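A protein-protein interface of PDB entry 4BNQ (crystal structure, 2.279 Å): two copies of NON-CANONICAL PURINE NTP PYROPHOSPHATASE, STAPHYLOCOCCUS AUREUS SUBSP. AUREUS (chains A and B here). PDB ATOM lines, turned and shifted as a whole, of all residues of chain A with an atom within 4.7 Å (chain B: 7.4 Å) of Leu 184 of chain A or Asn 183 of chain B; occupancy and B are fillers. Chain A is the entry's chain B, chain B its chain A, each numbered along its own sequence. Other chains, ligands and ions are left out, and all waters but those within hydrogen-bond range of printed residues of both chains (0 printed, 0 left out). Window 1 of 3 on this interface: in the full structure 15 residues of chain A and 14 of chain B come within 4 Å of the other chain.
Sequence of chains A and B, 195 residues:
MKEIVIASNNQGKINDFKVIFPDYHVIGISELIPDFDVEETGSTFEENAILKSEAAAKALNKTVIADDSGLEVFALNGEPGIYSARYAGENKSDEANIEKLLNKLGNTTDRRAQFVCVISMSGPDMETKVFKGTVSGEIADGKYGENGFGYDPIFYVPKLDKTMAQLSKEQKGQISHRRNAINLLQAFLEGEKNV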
ATOM      1  N   PHE A 131       8.431  13.551  11.491  1.00  0.00           N
ATOM      2  CA  PHE A 131       8.930  14.045  12.764  1.00  0.00           C
ATOM      3  C   PHE A 131       8.623  15.532  12.861  1.00  0.00           C
ATOM      4  O   PHE A 131       9.170  16.334  12.106  1.00  0.00           O
ATOM      5  CB  PHE A 131      10.435  13.823  12.861  1.00  0.00           C
ATOM      6  CG  PHE A 131      10.857  12.402  12.586  1.00  0.00           C
ATOM      7  CD1 PHE A 131      10.672  11.409  13.543  1.00  0.00           C
ATOM      8  CD2 PHE A 131      11.434  12.055  11.371  1.00  0.00           C
ATOM      9  CE1 PHE A 131      11.052  10.096  13.292  1.00  0.00           C
ATOM     10  CE2 PHE A 131      11.819  10.740  11.110  1.00  0.00           C
ATOM     11  CZ  PHE A 131      11.626   9.760  12.074  1.00  0.00           C
ATOM     12  N   LYS A 132       7.751  15.901  13.791  1.00  0.00           N
ATOM     13  CA  LYS A 132       7.246  17.268  13.858  1.00  0.00           C
ATOM     14  C   LYS A 132       7.800  18.018  15.063  1.00  0.00           C
ATOM     15  O   LYS A 132       7.678  17.580  16.207  1.00  0.00           O
ATOM     16  CB  LYS A 132       5.724  17.234  13.916  1.00  0.00           C
ATOM     17  CG  LYS A 132       5.054  18.557  14.187  1.00  0.00           C
ATOM     18  CD  LYS A 132       3.564  18.412  13.889  1.00  0.00           C
ATOM     19  CE  LYS A 132       2.766  19.608  14.361  1.00  0.00           C
ATOM     20  NZ  LYS A 132       1.418  19.586  13.719  1.00  0.00           N
ATOM     21  N   ASN A 180      13.728  20.758  17.371  1.00  0.00           N
ATOM     22  CA  ASN A 180      12.744  19.822  17.895  1.00  0.00           C
ATOM     23  C   ASN A 180      12.460  18.660  16.941  1.00  0.00           C
ATOM     24  O   ASN A 180      12.376  17.515  17.373  1.00  0.00           O
ATOM     25  CB  ASN A 180      11.468  20.552  18.335  1.00  0.00           C
ATOM     26  CG  ASN A 180      11.654  21.269  19.656  1.00  0.00           C
ATOM     27  OD1 ASN A 180      12.569  20.941  20.416  1.00  0.00           O
ATOM     28  ND2 ASN A 180      10.802  22.245  19.940  1.00  0.00           N
ATOM     29  N   ALA A 181      12.338  18.945  15.647  1.00  0.00           N
ATOM     30  CA  ALA A 181      12.095  17.871  14.680  1.00  0.00           C
ATOM     31  C   ALA A 181      13.327  16.988  14.525  1.00  0.00           C
ATOM     32  O   ALA A 181      13.219  15.768  14.448  1.00  0.00           O
ATOM     33  CB  ALA A 181      11.651  18.429  13.328  1.00  0.00           C
ATOM     34  N   ILE A 182      14.500  17.604  14.501  1.00  0.00           N
ATOM     35  CA  ILE A 182      15.744  16.849  14.392  1.00  0.00           C
ATOM     36  C   ILE A 182      15.983  15.931  15.593  1.00  0.00           C
ATOM     37  O   ILE A 182      16.498  14.820  15.435  1.00  0.00           O
ATOM     38  CB  ILE A 182      16.947  17.791  14.153  1.00  0.00           C
ATOM     39  CG1 ILE A 182      16.926  18.284  12.703  1.00  0.00           C
ATOM     40  CG2 ILE A 182      18.264  17.094  14.438  1.00  0.00           C
ATOM     41  CD1 ILE A 182      18.174  19.016  12.310  1.00  0.00           C
ATOM     42  N   ASN A 183      15.601  16.380  16.788  1.00  0.00           N
ATOM     43  CA  ASN A 183      15.733  15.547  17.981  1.00  0.00           C
ATOM     44  C   ASN A 183      14.914  14.295  17.812  1.00  0.00           C
ATOM     45  O   ASN A 183      15.343  13.216  18.195  1.00  0.00           O
ATOM     46  CB  ASN A 183      15.249  16.275  19.237  1.00  0.00           C
ATOM     47  CG  ASN A 183      16.144  17.433  19.635  1.00  0.00           C
ATOM     48  OD1 ASN A 183      17.307  17.514  19.223  1.00  0.00           O
ATOM     49  ND2 ASN A 183      15.603  18.339  20.459  1.00  0.00           N
ATOM     50  N   LEU A 184      13.725  14.445  17.243  1.00  0.00           N
ATOM     51  CA  LEU A 184      12.854  13.308  17.059  1.00  0.00           C
ATOM     52  C   LEU A 184      13.456  12.360  16.036  1.00  0.00           C
ATOM     53  O   LEU A 184      13.378  11.148  16.197  1.00  0.00           O
ATOM     54  CB  LEU A 184      11.446  13.754  16.660  1.00  0.00           C
ATOM     55  CG  LEU A 184      10.666  14.371  17.820  1.00  0.00           C
ATOM     56  CD1 LEU A 184       9.607  15.303  17.300  1.00  0.00           C
ATOM     57  CD2 LEU A 184      10.033  13.265  18.682  1.00  0.00           C
ATOM     58  N   LEU A 185      14.078  12.914  14.997  1.00  0.00           N
ATOM     59  CA  LEU A 185      14.736  12.103  13.978  1.00  0.00           C
ATOM     60  C   LEU A 185      15.903  11.337  14.577  1.00  0.00           C
ATOM     61  O   LEU A 185      16.001  10.123  14.411  1.00  0.00           O
ATOM     62  CB  LEU A 185      15.222  12.975  12.817  1.00  0.00           C
ATOM     63  CG  LEU A 185      16.068  12.325  11.709  1.00  0.00           C
ATOM     64  CD1 LEU A 185      15.306  11.212  11.010  1.00  0.00           C
ATOM     65  CD2 LEU A 185      16.502  13.380  10.692  1.00  0.00           C
ATOM     66  N   GLN A 186      16.781  12.049  15.278  1.00  0.00           N
ATOM     67  CA  GLN A 186      17.929  11.413  15.919  1.00  0.00           C
ATOM     68  C   GLN A 186      17.540  10.261  16.841  1.00  0.00           C
ATOM     69  O   GLN A 186      18.238   9.249  16.886  1.00  0.00           O
ATOM     70  CB  GLN A 186      18.766  12.441  16.681  1.00  0.00           C
ATOM     71  CG  GLN A 186      19.720  13.221  15.794  1.00  0.00           C
ATOM     72  CD  GLN A 186      20.681  14.079  16.583  1.00  0.00           C
ATOM     73  OE1 GLN A 186      20.302  15.107  17.161  1.00  0.00           O
ATOM     74  NE2 GLN A 186      21.941  13.665  16.610  1.00  0.00           N
ATOM     75  N   ALA A 187      16.425  10.410  17.558  1.00  0.00           N
ATOM     76  CA  ALA A 187      15.960   9.370  18.478  1.00  0.00           C
ATOM     77  C   ALA A 187      15.537   8.122  17.708  1.00  0.00           C
ATOM     78  O   ALA A 187      15.759   6.993  18.161  1.00  0.00           O
ATOM     79  CB  ALA A 187      14.816   9.882  19.348  1.00  0.00           C
ATOM     80  N   PHE A 188      14.925   8.339  16.547  1.00  0.00           N
ATOM     81  CA  PHE A 188      14.580   7.264  15.634  1.00  0.00           C
ATOM     82  C   PHE A 188      15.843   6.565  15.160  1.00  0.00           C
ATOM     83  O   PHE A 188      15.935   5.338  15.193  1.00  0.00           O
ATOM     84  CB  PHE A 188      13.840   7.827  14.423  1.00  0.00           C
ATOM     85  CG  PHE A 188      13.434   6.786  13.418  1.00  0.00           C
ATOM     86  CD1 PHE A 188      14.283   6.421  12.379  1.00  0.00           C
ATOM     87  CD2 PHE A 188      12.195   6.167  13.508  1.00  0.00           C
ATOM     88  CE1 PHE A 188      13.900   5.445  11.448  1.00  0.00           C
ATOM     89  CE2 PHE A 188      11.808   5.197  12.580  1.00  0.00           C
ATOM     90  CZ  PHE A 188      12.663   4.841  11.549  1.00  0.00           C
ATOM     91  N   ILE B  20      -1.259   9.072  27.291  1.00  0.00           N
ATOM     92  CA  ILE B  20      -0.212   9.142  26.269  1.00  0.00           C
ATOM     93  C   ILE B  20       0.064   7.809  25.561  1.00  0.00           C
ATOM     94  O   ILE B  20       0.575   7.794  24.451  1.00  0.00           O
ATOM     95  CB  ILE B  20       1.093   9.683  26.909  1.00  0.00           C
ATOM     96  CG1 ILE B  20       0.981  11.186  27.146  1.00  0.00           C
ATOM     97  CG2 ILE B  20       2.307   9.445  26.040  1.00  0.00           C
ATOM     98  CD1 ILE B  20       1.984  11.663  28.191  1.00  0.00           C
ATOM     99  N   PHE B  21      -0.270   6.686  26.196  1.00  0.00           N
ATOM    100  CA  PHE B  21      -0.157   5.375  25.548  1.00  0.00           C
ATOM    101  C   PHE B  21      -1.521   4.702  25.479  1.00  0.00           C
ATOM    102  O   PHE B  21      -1.734   3.709  26.175  1.00  0.00           O
ATOM    103  CB  PHE B  21       0.728   4.434  26.368  1.00  0.00           C
ATOM    104  CG  PHE B  21       2.189   4.810  26.420  1.00  0.00           C
ATOM    105  CD1 PHE B  21       3.019   4.633  25.322  1.00  0.00           C
ATOM    106  CD2 PHE B  21       2.746   5.273  27.595  1.00  0.00           C
ATOM    107  CE1 PHE B  21       4.377   4.948  25.394  1.00  0.00           C
ATOM    108  CE2 PHE B  21       4.104   5.587  27.670  1.00  0.00           C
ATOM    109  CZ  PHE B  21       4.916   5.419  26.578  1.00  0.00           C
ATOM    110  N   ILE B 119      12.631  10.647  30.978  1.00  0.00           N
ATOM    111  CA  ILE B 119      12.173   9.259  30.958  1.00  0.00           C
ATOM    112  C   ILE B 119      13.392   8.372  30.731  1.00  0.00           C
ATOM    113  O   ILE B 119      14.135   8.597  29.779  1.00  0.00           O
ATOM    114  CB  ILE B 119      11.206   9.034  29.782  1.00  0.00           C
ATOM    115  CG1 ILE B 119       9.943   9.885  29.945  1.00  0.00           C
ATOM    116  CG2 ILE B 119      10.809   7.563  29.646  1.00  0.00           C
ATOM    117  CD1 ILE B 119       9.031   9.464  31.096  1.00  0.00           C
ATOM    118  N   PHE B 131      15.503  10.033  27.869  1.00  0.00           N
ATOM    119  CA  PHE B 131      14.888  11.010  26.969  1.00  0.00           C
ATOM    120  C   PHE B 131      14.298  12.189  27.745  1.00  0.00           C
ATOM    121  O   PHE B 131      13.575  11.993  28.725  1.00  0.00           O
ATOM    122  CB  PHE B 131      13.774  10.352  26.164  1.00  0.00           C
ATOM    123  CG  PHE B 131      14.178   9.066  25.507  1.00  0.00           C
ATOM    124  CD1 PHE B 131      14.125   7.864  26.200  1.00  0.00           C
ATOM    125  CD2 PHE B 131      14.604   9.051  24.196  1.00  0.00           C
ATOM    126  CE1 PHE B 131      14.484   6.678  25.586  1.00  0.00           C
ATOM    127  CE2 PHE B 131      14.971   7.860  23.588  1.00  0.00           C
ATOM    128  CZ  PHE B 131      14.910   6.682  24.273  1.00  0.00           C
ATOM    129  N   GLY B 173      -2.044  15.984  27.809  1.00  0.00           N
ATOM    130  CA  GLY B 173      -1.280  14.977  27.101  1.00  0.00           C
ATOM    131  C   GLY B 173      -0.784  15.367  25.719  1.00  0.00           C
ATOM    132  O   GLY B 173       0.039  14.666  25.141  1.00  0.00           O
ATOM    133  N   GLN B 174      -1.281  16.468  25.176  1.00  0.00           N
ATOM    134  CA  GLN B 174      -0.834  16.928  23.871  1.00  0.00           C
ATOM    135  C   GLN B 174       0.396  17.819  24.009  1.00  0.00           C
ATOM    136  O   GLN B 174       1.162  17.980  23.057  1.00  0.00           O
ATOM    137  CB  GLN B 174      -1.945  17.733  23.183  1.00  0.00           C
ATOM    138  CG  GLN B 174      -3.192  16.942  22.798  1.00  0.00           C
ATOM    139  CD  GLN B 174      -2.897  15.818  21.821  1.00  0.00           C
ATOM    140  OE1 GLN B 174      -2.733  16.045  20.617  1.00  0.00           O
ATOM    141  NE2 GLN B 174      -2.815  14.591  22.338  1.00  0.00           N
ATOM    142  N   SER B 176       2.357  18.432  27.381  1.00  0.00           N
ATOM    143  CA  SER B 176       3.165  18.416  28.591  1.00  0.00           C
ATOM    144  C   SER B 176       4.611  18.051  28.282  1.00  0.00           C
ATOM    145  O   SER B 176       4.917  17.495  27.226  1.00  0.00           O
ATOM    146  CB  SER B 176       2.599  17.432  29.616  1.00  0.00           C
ATOM    147  OG  SER B 176       2.883  16.089  29.221  1.00  0.00           O
ATOM    148  N   HIS B 177       5.489  18.379  29.222  1.00  0.00           N
ATOM    149  CA  HIS B 177       6.888  17.972  29.209  1.00  0.00           C
ATOM    150  C   HIS B 177       7.040  16.447  29.113  1.00  0.00           C
ATOM    151  O   HIS B 177       7.976  15.937  28.487  1.00  0.00           O
ATOM    152  CB  HIS B 177       7.583  18.508  30.470  1.00  0.00           C
ATOM    153  CG  HIS B 177       6.889  18.158  31.751  1.00  0.00           C
ATOM    154  ND1 HIS B 177       5.554  18.486  31.986  1.00  0.00           N
ATOM    155  CD2 HIS B 177       7.313  17.528  32.850  1.00  0.00           C
ATOM    156  CE1 HIS B 177       5.217  18.054  33.180  1.00  0.00           C
ATOM    157  NE2 HIS B 177       6.259  17.478  33.742  1.00  0.00           N
ATOM    158  N   ARG B 178       6.111  15.733  29.733  1.00  0.00           N
ATOM    159  CA  ARG B 178       6.117  14.280  29.710  1.00  0.00           C
ATOM    160  C   ARG B 178       5.686  13.781  28.325  1.00  0.00           C
ATOM    161  O   ARG B 178       6.228  12.810  27.829  1.00  0.00           O
ATOM    162  CB  ARG B 178       5.198  13.744  30.803  1.00  0.00           C
ATOM    163  CG  ARG B 178       5.213  12.233  31.001  1.00  0.00           C
ATOM    164  CD  ARG B 178       4.969  11.857  32.484  1.00  0.00           C
ATOM    165  NE  ARG B 178       4.181  12.859  33.168  1.00  0.00           N
ATOM    166  CZ  ARG B 178       4.590  13.585  34.200  1.00  0.00           C
ATOM    167  NH1 ARG B 178       5.795  13.411  34.739  1.00  0.00           N
ATOM    168  NH2 ARG B 178       3.771  14.497  34.692  1.00  0.00           N
ATOM    169  N   ARG B 179       4.720  14.446  27.700  1.00  0.00           N
ATOM    170  CA  ARG B 179       4.369  14.107  26.324  1.00  0.00           C
ATOM    171  C   ARG B 179       5.581  14.279  25.425  1.00  0.00           C
ATOM    172  O   ARG B 179       5.840  13.441  24.564  1.00  0.00           O
ATOM    173  CB  ARG B 179       3.216  14.968  25.809  1.00  0.00           C
ATOM    174  CG  ARG B 179       2.978  14.824  24.311  1.00  0.00           C
ATOM    175  CD  ARG B 179       2.602  13.393  23.947  1.00  0.00           C
ATOM    176  NE  ARG B 179       2.635  13.159  22.508  1.00  0.00           N
ATOM    177  CZ  ARG B 179       1.556  13.088  21.741  1.00  0.00           C
ATOM    178  NH1 ARG B 179       0.353  13.233  22.281  1.00  0.00           N
ATOM    179  NH2 ARG B 179       1.680  12.874  20.438  1.00  0.00           N
ATOM    180  N   ASN B 180       6.338  15.351  25.634  1.00  0.00           N
ATOM    181  CA  ASN B 180       7.486  15.624  24.770  1.00  0.00           C
ATOM    182  C   ASN B 180       8.599  14.600  24.935  1.00  0.00           C
ATOM    183  O   ASN B 180       9.224  14.214  23.957  1.00  0.00           O
ATOM    184  CB  ASN B 180       8.040  17.036  24.998  1.00  0.00           C
ATOM    185  CG  ASN B 180       7.170  18.097  24.377  1.00  0.00           C
ATOM    186  OD1 ASN B 180       6.407  17.819  23.455  1.00  0.00           O
ATOM    187  ND2 ASN B 180       7.265  19.319  24.883  1.00  0.00           N
ATOM    188  N   ALA B 181       8.848  14.172  26.170  1.00  0.00           N
ATOM    189  CA  ALA B 181       9.841  13.141  26.428  1.00  0.00           C
ATOM    190  C   ALA B 181       9.431  11.825  25.799  1.00  0.00           C
ATOM    191  O   ALA B 181      10.262  11.108  25.250  1.00  0.00           O
ATOM    192  CB  ALA B 181      10.016  12.946  27.913  1.00  0.00           C
ATOM    193  N   ILE B 182       8.153  11.486  25.920  1.00  0.00           N
ATOM    194  CA  ILE B 182       7.668  10.215  25.415  1.00  0.00           C
ATOM    195  C   ILE B 182       7.716  10.186  23.883  1.00  0.00           C
ATOM    196  O   ILE B 182       7.918   9.121  23.305  1.00  0.00           O
ATOM    197  CB  ILE B 182       6.241   9.909  25.910  1.00  0.00           C
ATOM    198  CG1 ILE B 182       6.246   9.635  27.405  1.00  0.00           C
ATOM    199  CG2 ILE B 182       5.668   8.684  25.203  1.00  0.00           C
ATOM    200  CD1 ILE B 182       6.971   8.351  27.798  1.00  0.00           C
ATOM    201  N   ASN B 183       7.563  11.347  23.236  1.00  0.00           N
ATOM    202  CA  ASN B 183       7.642  11.425  21.763  1.00  0.00           C
ATOM    203  C   ASN B 183       9.013  10.991  21.272  1.00  0.00           C
ATOM    204  O   ASN B 183       9.126  10.282  20.268  1.00  0.00           O
ATOM    205  CB  ASN B 183       7.325  12.834  21.235  1.00  0.00           C
ATOM    206  CG  ASN B 183       5.837  13.153  21.250  1.00  0.00           C
ATOM    207  OD1 ASN B 183       4.989  12.252  21.292  1.00  0.00           O
ATOM    208  ND2 ASN B 183       5.512  14.447  21.203  1.00  0.00           N
ATOM    209  N   LEU B 184      10.047  11.407  21.998  1.00  0.00           N
ATOM    210  CA  LEU B 184      11.406  10.963  21.716  1.00  0.00           C
ATOM    211  C   LEU B 184      11.533   9.463  21.979  1.00  0.00           C
ATOM    212  O   LEU B 184      12.214   8.752  21.230  1.00  0.00           O
ATOM    213  CB  LEU B 184      12.432  11.741  22.549  1.00  0.00           C
ATOM    214  CG  LEU B 184      12.580  13.246  22.282  1.00  0.00           C
ATOM    215  CD1 LEU B 184      13.329  13.935  23.440  1.00  0.00           C
ATOM    216  CD2 LEU B 184      13.298  13.489  20.959  1.00  0.00           C
ATOM    217  N   LEU B 185      10.862   8.971  23.021  1.00  0.00           N
ATOM    218  CA  LEU B 185      10.887   7.531  23.317  1.00  0.00           C
ATOM    219  C   LEU B 185      10.218   6.743  22.202  1.00  0.00           C
ATOM    220  O   LEU B 185      10.786   5.775  21.697  1.00  0.00           O
ATOM    221  CB  LEU B 185      10.183   7.209  24.637  1.00  0.00           C
ATOM    222  CG  LEU B 185       9.987   5.709  24.921  1.00  0.00           C
ATOM    223  CD1 LEU B 185      11.345   5.040  25.117  1.00  0.00           C
ATOM    224  CD2 LEU B 185       9.099   5.466  26.156  1.00  0.00           C
ATOM    225  N   GLN B 186       9.004   7.148  21.837  1.00  0.00           N
ATOM    226  CA  GLN B 186       8.244   6.439  20.814  1.00  0.00           C
ATOM    227  C   GLN B 186       8.955   6.452  19.478  1.00  0.00           C
ATOM    228  O   GLN B 186       8.889   5.468  18.735  1.00  0.00           O
ATOM    229  CB  GLN B 186       6.814   6.985  20.702  1.00  0.00           C
ATOM    230  CG  GLN B 186       5.892   6.385  21.765  1.00  0.00           C
ATOM    231  CD  GLN B 186       4.557   7.079  21.843  1.00  0.00           C
ATOM    232  OE1 GLN B 186       4.408   8.222  21.397  1.00  0.00           O
ATOM    233  NE2 GLN B 186       3.569   6.394  22.403  1.00  0.00           N
ATOM    234  N   ALA B 187       9.651   7.551  19.185  1.00  0.00           N
ATOM    235  CA  ALA B 187      10.450   7.628  17.961  1.00  0.00           C
ATOM    236  C   ALA B 187      11.592   6.626  18.033  1.00  0.00           C
ATOM    237  O   ALA B 187      11.926   5.986  17.042  1.00  0.00           O
ATOM    238  CB  ALA B 187      10.988   9.038  17.730  1.00  0.00           C
ATOM    239  N   PHE B 188      12.192   6.507  19.213  1.00  0.00           N
ATOM    240  CA  PHE B 188      13.244   5.533  19.449  1.00  0.00           C
ATOM    241  C   PHE B 188      12.731   4.105  19.197  1.00  0.00           C
ATOM    242  O   PHE B 188      13.379   3.312  18.515  1.00  0.00           O
ATOM    243  CB  PHE B 188      13.764   5.679  20.881  1.00  0.00           C
ATOM    244  CG  PHE B 188      14.871   4.723  21.229  1.00  0.00           C
ATOM    245  CD1 PHE B 188      14.587   3.458  21.748  1.00  0.00           C
ATOM    246  CD2 PHE B 188      16.196   5.083  21.044  1.00  0.00           C
ATOM    247  CE1 PHE B 188      15.613   2.569  22.068  1.00  0.00           C
ATOM    248  CE2 PHE B 188      17.225   4.202  21.365  1.00  0.00           C
ATOM    249  CZ  PHE B 188      16.931   2.942  21.881  1.00  0.00           C
ATOM    250  N   LEU B 189      11.568   3.793  19.757  1.00  0.00           N
ATOM    251  CA  LEU B 189      10.932   2.492  19.570  1.00  0.00           C
ATOM    252  C   LEU B 189      10.610   2.215  18.096  1.00  0.00           C
ATOM    253  O   LEU B 189      10.752   1.085  17.616  1.00  0.00           O
ATOM    254  CB  LEU B 189       9.643   2.408  20.391  1.00  0.00           C
ATOM    255  CG  LEU B 189       9.771   2.598  21.909  1.00  0.00           C
ATOM    256  CD1 LEU B 189       8.389   2.607  22.576  1.00  0.00           C
ATOM    257  CD2 LEU B 189      10.630   1.509  22.494  1.00  0.00           C
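Asn 183 of chain A touches Leu 184 of chain B, and with the chains exchanged Leu 184 of chain A touches Asn 183 of chain B. Leu 184 of chain B touches its own counterpart, Leu 184 of chain A. Leu 184 of chain A touches Ala 187 of chain B, and with the chains exchanged Ala 187 of chain A touches Leu 184 of chain B. Ala 187 of chain A touches Phe 188 of chain B, and with the chains exchanged Phe 188 of chain A touches Ala 187 of chain B. Positions printed for both chains: 131, 180, 181, 182, 183, 184, 185, 186, 187 and 188.
Asn 183 of chain A touches Leu 184 of chain B. CD2 of Leu 184 of chain A touches O of Asn 183 of chain B, 3.5 Å away. Leu 184 of chain B touches Leu 184 of chain A (N to CD2, 3.8 Å). O of Leu 184 of chain A touches CB of Ala 187 of chain B (3.5 Å). CB of Ala 187 of chain A touches O of Leu 184 of chain B, at 3.4 Å. Ala 187 of chain A touches Phe 188 of chain B. Phe 188 of chain A touches Ala 187 of chain B.
NE of Arg 179 of chain B is in hydrogen-bond range of OD1 of Asn 183 of chain B (2.8 Å).
Printed residues of chain B within 4 Å of Asn 183 of chain A: Leu 184. Leu 184 of chain A touches just these residues of chain B: Asn 183, Leu 184 and Ala 187. Printed residues of chain B within 4 Å of Ala 187 of chain A: Leu 184 (3.4 Å) and Phe 188 (3.2 Å). Printed residues of chain B within 4 Å of Phe 188 of chain A: Ala 187 (3.3 Å). Gln 174 of chain B touches none of the printed residues of chain A. Asn 183 of chain B touches just one residue of chain A: Leu 184. Of the printed residues of chain A, Leu 184 of chain B touches Asn 183 (3.4 Å), Leu 184 (3.8 Å) and Ala 187 (3.4 Å). Of the printed residues of chain A, Phe 188 of chain B touches Ala 187 (3.2 Å). The nearest printed residue of chain A that does not touch Asn 183 of chain B is Ala 187 of chain A (5.8 Å). The nearest printed residue of chain A that does not touch Phe 188 of chain B is Phe 188 of chain A (4.2 Å).
Of the 20 printed residues of chain B, 4 touch a printed residue of chain A. Hydrophobic or aromatic side chains of chain B within 4 Å of the printed part of chain A: Leu 184, Ala 187 and Phe 188. Of the 11 printed residues of chain A, 4 touch a printed residue of chain B. Hydrophobic or aromatic side chains of chain A that line the printed part of chain B: Leu 184, Ala 187 and Phe 188.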
